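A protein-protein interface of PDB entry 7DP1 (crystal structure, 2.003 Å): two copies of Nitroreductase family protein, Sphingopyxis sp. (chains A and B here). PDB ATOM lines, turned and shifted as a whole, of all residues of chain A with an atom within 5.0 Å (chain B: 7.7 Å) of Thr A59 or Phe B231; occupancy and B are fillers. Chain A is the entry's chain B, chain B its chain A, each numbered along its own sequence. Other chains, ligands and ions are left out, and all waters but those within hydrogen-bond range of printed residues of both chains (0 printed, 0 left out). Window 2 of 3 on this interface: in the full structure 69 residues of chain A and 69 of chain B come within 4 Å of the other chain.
The backbone NH (N) of Val A57 is in hydrogen-bond range of the backbone carbonyl oxygen (O) of Asp B227 (2.6 Å). The backbone carbonyl oxygen (O) of Val A57 lies within hydrogen-bond range of the backbone NH (N) of Gln B229 (2.8 Å). The backbone carbonyl oxygen (O) of Gln B229 lies within hydrogen-bond range of the backbone NH (N) of Thr A59 (3.0 Å).
The side-chain carboxylate (OD2) of Asp B227 is in hydrogen-bond range of the side-chain amide nitrogen (NE2) of Gln B229. OG1 of Thr A59 lies within hydrogen-bond range of O of Pro A135, 2.7 Å away.
NH2 of Arg A31 touches CD1 of Trp B228 (3.6 Å). Phe B231 touches Arg A31 (CD1 to CD, 3.9 Å). CA of Trp B228 touches O of Val A57, at 3.5 Å. Val A57 touches Phe B231 (O to CE2, 3.4 Å). Val A58 touches Gln B229 (CA to O, 3.2 Å). Thr A59 touches Gly B230 (CG2 to O, 3.4 Å). Phe B231 touches Thr A59. Arg A62 touches Gln B229 (NH1 to OE1, 3.7 Å). CG of Arg A62 touches N of Gly B230 (3.6 Å).
Phe B231 touches three residues of chain A. No residue of chain B comes within 4 Å of Gly A60. Printed residues of chain A within 4 Å of Gly B230: Thr A59 and Arg A62. Printed residues of chain B within 4 Å of Val A57: Asp B227 (2.6 Å), Trp B228 (3.5 Å), Gln B229 (2.8 Å) and Phe B231 (3.4 Å). Of the printed residues of chain A, Gln B229 touches Val A57 (2.8 Å), Val A58 (3.2 Å), Thr A59 (3.0 Å) and Arg A62 (3.7 Å). Printed residues of chain A within 4 Å of Trp B228: Arg A31 (3.6 Å) and Val A57 (3.5 Å). Of the printed residues of chain B, Arg A62 touches Gln B229 and Gly B230. The nearest residue of chain B that does not touch Thr A59 is Trp B228 (6.7 Å).
Printed residues of chain A that touch a printed residue of chain B: Arg A31, Val A57, Val A58, Thr A59 and Arg A62. Along chain A the printed residues that touch a printed residue of chain B span positions 31 to 62. Among the printed residues, no Asp or Glu carboxylate lies within 4 Å of a Lys or Arg side-chain nitrogen of the other chain.
No position is printed for both chains. Of the 12 pairs that touch across the chains among the printed residues, none has its exchanged pair printed and touching as well.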
ATOM      1  N   ARG A  31     -30.947   5.599 -11.405  1.00  0.00           N
ATOM      2  CA  ARG A  31     -29.862   5.120 -12.262  1.00  0.00           C
ATOM      3  C   ARG A  31     -29.349   6.220 -13.193  1.00  0.00           C
ATOM      4  O   ARG A  31     -28.145   6.318 -13.442  1.00  0.00           O
ATOM      5  CB  ARG A  31     -30.276   3.878 -13.054  1.00  0.00           C
ATOM      6  CG  ARG A  31     -29.192   3.399 -14.037  1.00  0.00           C
ATOM      7  CD  ARG A  31     -29.683   2.248 -14.905  1.00  0.00           C
ATOM      8  NE  ARG A  31     -28.622   1.670 -15.731  1.00  0.00           N
ATOM      9  CZ  ARG A  31     -28.193   2.192 -16.878  1.00  0.00           C
ATOM     10  NH1 ARG A  31     -28.744   3.303 -17.348  1.00  0.00           N
ATOM     11  NH2 ARG A  31     -27.230   1.591 -17.569  1.00  0.00           N
ATOM     12  N   LEU A  34     -26.953   8.418 -11.178  1.00  0.00           N
ATOM     13  CA  LEU A  34     -25.651   7.773 -10.963  1.00  0.00           C
ATOM     14  C   LEU A  34     -24.786   7.867 -12.206  1.00  0.00           C
ATOM     15  O   LEU A  34     -23.589   8.173 -12.129  1.00  0.00           O
ATOM     16  CB  LEU A  34     -25.796   6.301 -10.584  1.00  0.00           C
ATOM     17  CG  LEU A  34     -26.054   5.865  -9.149  1.00  0.00           C
ATOM     18  CD1 LEU A  34     -25.902   4.353  -9.069  1.00  0.00           C
ATOM     19  CD2 LEU A  34     -25.137   6.563  -8.150  1.00  0.00           C
ATOM     20  N   VAL A  57     -21.205  -1.830 -11.023  1.00  0.00           N
ATOM     21  CA  VAL A  57     -22.260  -1.351 -10.141  1.00  0.00           C
ATOM     22  C   VAL A  57     -23.401  -2.365 -10.076  1.00  0.00           C
ATOM     23  O   VAL A  57     -23.977  -2.733 -11.102  1.00  0.00           O
ATOM     24  CB  VAL A  57     -22.768   0.020 -10.621  1.00  0.00           C
ATOM     25  CG1 VAL A  57     -23.764   0.583  -9.658  1.00  0.00           C
ATOM     26  CG2 VAL A  57     -21.586   0.975 -10.755  1.00  0.00           C
ATOM     27  N   VAL A  58     -23.719  -2.857  -8.885  1.00  0.00           N
ATOM     28  CA  VAL A  58     -24.784  -3.858  -8.798  1.00  0.00           C
ATOM     29  C   VAL A  58     -25.944  -3.413  -7.922  1.00  0.00           C
ATOM     30  O   VAL A  58     -25.794  -2.594  -7.025  1.00  0.00           O
ATOM     31  CB  VAL A  58     -24.257  -5.210  -8.274  1.00  0.00           C
ATOM     32  CG1 VAL A  58     -23.101  -5.691  -9.127  1.00  0.00           C
ATOM     33  CG2 VAL A  58     -23.803  -5.091  -6.832  1.00  0.00           C
ATOM     34  N   THR A  59     -27.119  -3.956  -8.215  1.00  0.00           N
ATOM     35  CA  THR A  59     -28.326  -3.694  -7.443  1.00  0.00           C
ATOM     36  C   THR A  59     -29.217  -4.917  -7.581  1.00  0.00           C
ATOM     37  O   THR A  59     -28.874  -5.864  -8.296  1.00  0.00           O
ATOM     38  CB  THR A  59     -29.088  -2.428  -7.909  1.00  0.00           C
ATOM     39  OG1 THR A  59     -30.117  -2.117  -6.955  1.00  0.00           O
ATOM     40  CG2 THR A  59     -29.759  -2.664  -9.276  1.00  0.00           C
ATOM     41  N   GLY A  60     -30.336  -4.907  -6.864  1.00  0.00           N
ATOM     42  CA  GLY A  60     -31.322  -5.973  -6.942  1.00  0.00           C
ATOM     43  C   GLY A  60     -30.814  -7.390  -6.755  1.00  0.00           C
ATOM     44  O   GLY A  60     -30.050  -7.681  -5.830  1.00  0.00           O
ATOM     45  N   GLU A  61     -31.245  -8.277  -7.641  1.00  0.00           N
ATOM     46  CA  GLU A  61     -30.976  -9.698  -7.491  1.00  0.00           C
ATOM     47  C   GLU A  61     -29.482 -10.002  -7.601  1.00  0.00           C
ATOM     48  O   GLU A  61     -28.966 -10.867  -6.892  1.00  0.00           O
ATOM     49  CB  GLU A  61     -31.788 -10.499  -8.513  1.00  0.00           C
ATOM     50  CG  GLU A  61     -33.291 -10.435  -8.241  1.00  0.00           C
ATOM     51  CD  GLU A  61     -34.116 -11.224  -9.236  1.00  0.00           C
ATOM     52  OE1 GLU A  61     -34.028 -10.935 -10.448  1.00  0.00           O
ATOM     53  OE2 GLU A  61     -34.862 -12.128  -8.804  1.00  0.00           O
ATOM     54  N   ARG A  62     -28.786  -9.305  -8.492  1.00  0.00           N
ATOM     55  CA  ARG A  62     -27.345  -9.504  -8.618  1.00  0.00           C
ATOM     56  C   ARG A  62     -26.627  -9.104  -7.335  1.00  0.00           C
ATOM     57  O   ARG A  62     -25.714  -9.794  -6.872  1.00  0.00           O
ATOM     58  CB  ARG A  62     -26.788  -8.716  -9.804  1.00  0.00           C
ATOM     59  CG  ARG A  62     -27.342  -9.174 -11.130  1.00  0.00           C
ATOM     60  CD  ARG A  62     -26.837 -10.557 -11.465  1.00  0.00           C
ATOM     61  NE  ARG A  62     -27.419 -11.061 -12.710  1.00  0.00           N
ATOM     62  CZ  ARG A  62     -26.923 -10.822 -13.921  1.00  0.00           C
ATOM     63  NH1 ARG A  62     -25.825 -10.093 -14.054  1.00  0.00           N
ATOM     64  NH2 ARG A  62     -27.523 -11.321 -14.996  1.00  0.00           N
ATOM     65  N   TRP A  63     -27.029  -7.959  -6.795  1.00  0.00           N
ATOM     66  CA  TRP A  63     -26.493  -7.443  -5.547  1.00  0.00           C
ATOM     67  C   TRP A  63     -26.781  -8.410  -4.397  1.00  0.00           C
ATOM     68  O   TRP A  63     -25.954  -8.589  -3.502  1.00  0.00           O
ATOM     69  CB  TRP A  63     -27.079  -6.048  -5.306  1.00  0.00           C
ATOM     70  CG  TRP A  63     -26.863  -5.374  -3.986  1.00  0.00           C
ATOM     71  CD1 TRP A  63     -27.739  -4.531  -3.366  1.00  0.00           C
ATOM     72  CD2 TRP A  63     -25.709  -5.445  -3.133  1.00  0.00           C
ATOM     73  NE1 TRP A  63     -27.212  -4.076  -2.184  1.00  0.00           N
ATOM     74  CE2 TRP A  63     -25.967  -4.619  -2.017  1.00  0.00           C
ATOM     75  CE3 TRP A  63     -24.479  -6.119  -3.206  1.00  0.00           C
ATOM     76  CZ2 TRP A  63     -25.060  -4.473  -0.973  1.00  0.00           C
ATOM     77  CZ3 TRP A  63     -23.583  -5.978  -2.170  1.00  0.00           C
ATOM     78  CH2 TRP A  63     -23.871  -5.154  -1.069  1.00  0.00           C
ATOM     79  N   PRO A 135     -29.151   0.157  -1.354  1.00  0.00           N
ATOM     80  CA  PRO A 135     -29.780  -0.508  -2.496  1.00  0.00           C
ATOM     81  C   PRO A 135     -28.798  -0.758  -3.636  1.00  0.00           C
ATOM     82  O   PRO A 135     -29.063  -1.575  -4.506  1.00  0.00           O
ATOM     83  CB  PRO A 135     -30.855   0.488  -2.934  1.00  0.00           C
ATOM     84  CG  PRO A 135     -30.301   1.787  -2.560  1.00  0.00           C
ATOM     85  CD  PRO A 135     -29.567   1.566  -1.258  1.00  0.00           C
ATOM     86  N   VAL A 136     -27.692  -0.023  -3.656  1.00  0.00           N
ATOM     87  CA  VAL A 136     -26.727  -0.151  -4.740  1.00  0.00           C
ATOM     88  C   VAL A 136     -25.325  -0.344  -4.160  1.00  0.00           C
ATOM     89  O   VAL A 136     -24.982   0.272  -3.153  1.00  0.00           O
ATOM     90  CB  VAL A 136     -26.740   1.079  -5.665  1.00  0.00           C
ATOM     91  CG1 VAL A 136     -25.551   1.047  -6.629  1.00  0.00           C
ATOM     92  CG2 VAL A 136     -28.045   1.152  -6.426  1.00  0.00           C
ATOM     93  N   ASP B 227     -19.654  -1.129 -15.461  1.00  0.00           N
ATOM     94  CA  ASP B 227     -20.534  -2.256 -15.778  1.00  0.00           C
ATOM     95  C   ASP B 227     -21.729  -2.237 -14.835  1.00  0.00           C
ATOM     96  O   ASP B 227     -21.566  -2.092 -13.626  1.00  0.00           O
ATOM     97  CB  ASP B 227     -19.781  -3.576 -15.664  1.00  0.00           C
ATOM     98  CG  ASP B 227     -20.616  -4.749 -16.073  1.00  0.00           C
ATOM     99  OD1 ASP B 227     -21.354  -4.636 -17.072  1.00  0.00           O
ATOM    100  OD2 ASP B 227     -20.541  -5.785 -15.388  1.00  0.00           O
ATOM    101  N   TRP B 228     -22.931  -2.331 -15.386  1.00  0.00           N
ATOM    102  CA  TRP B 228     -24.145  -2.314 -14.588  1.00  0.00           C
ATOM    103  C   TRP B 228     -24.752  -3.703 -14.483  1.00  0.00           C
ATOM    104  O   TRP B 228     -24.887  -4.397 -15.487  1.00  0.00           O
ATOM    105  CB  TRP B 228     -25.171  -1.345 -15.187  1.00  0.00           C
ATOM    106  CG  TRP B 228     -24.641   0.041 -15.507  1.00  0.00           C
ATOM    107  CD1 TRP B 228     -23.926   0.414 -16.612  1.00  0.00           C
ATOM    108  CD2 TRP B 228     -24.796   1.227 -14.715  1.00  0.00           C
ATOM    109  NE1 TRP B 228     -23.626   1.751 -16.554  1.00  0.00           N
ATOM    110  CE2 TRP B 228     -24.148   2.273 -15.400  1.00  0.00           C
ATOM    111  CE3 TRP B 228     -25.409   1.505 -13.489  1.00  0.00           C
ATOM    112  CZ2 TRP B 228     -24.104   3.570 -14.905  1.00  0.00           C
ATOM    113  CZ3 TRP B 228     -25.366   2.800 -13.004  1.00  0.00           C
ATOM    114  CH2 TRP B 228     -24.724   3.812 -13.710  1.00  0.00           C
ATOM    115  N   GLN B 229     -25.167  -4.098 -13.285  1.00  0.00           N
ATOM    116  CA  GLN B 229     -25.755  -5.428 -13.108  1.00  0.00           C
ATOM    117  C   GLN B 229     -26.955  -5.401 -12.173  1.00  0.00           C
ATOM    118  O   GLN B 229     -26.883  -4.855 -11.068  1.00  0.00           O
ATOM    119  CB  GLN B 229     -24.720  -6.407 -12.566  1.00  0.00           C
ATOM    120  CG  GLN B 229     -23.610  -6.740 -13.532  1.00  0.00           C
ATOM    121  CD  GLN B 229     -22.686  -7.791 -12.978  1.00  0.00           C
ATOM    122  OE1 GLN B 229     -23.064  -8.552 -12.089  1.00  0.00           O
ATOM    123  NE2 GLN B 229     -21.461  -7.833 -13.483  1.00  0.00           N
ATOM    124  N   GLY B 230     -28.057  -5.993 -12.630  1.00  0.00           N
ATOM    125  CA  GLY B 230     -29.263  -6.114 -11.834  1.00  0.00           C
ATOM    126  C   GLY B 230     -30.212  -4.941 -11.967  1.00  0.00           C
ATOM    127  O   GLY B 230     -31.245  -4.898 -11.304  1.00  0.00           O
ATOM    128  N   PHE B 231     -29.883  -3.993 -12.839  1.00  0.00           N
ATOM    129  CA  PHE B 231     -30.751  -2.836 -13.036  1.00  0.00           C
ATOM    130  C   PHE B 231     -31.833  -3.140 -14.054  1.00  0.00           C
ATOM    131  O   PHE B 231     -31.531  -3.591 -15.152  1.00  0.00           O
ATOM    132  CB  PHE B 231     -29.948  -1.627 -13.494  1.00  0.00           C
ATOM    133  CG  PHE B 231     -29.060  -1.074 -12.444  1.00  0.00           C
ATOM    134  CD1 PHE B 231     -29.448   0.028 -11.713  1.00  0.00           C
ATOM    135  CD2 PHE B 231     -27.848  -1.681 -12.152  1.00  0.00           C
ATOM    136  CE1 PHE B 231     -28.626   0.531 -10.728  1.00  0.00           C
ATOM    137  CE2 PHE B 231     -27.042  -1.182 -11.170  1.00  0.00           C
ATOM    138  CZ  PHE B 231     -27.434  -0.085 -10.452  1.00  0.00           C
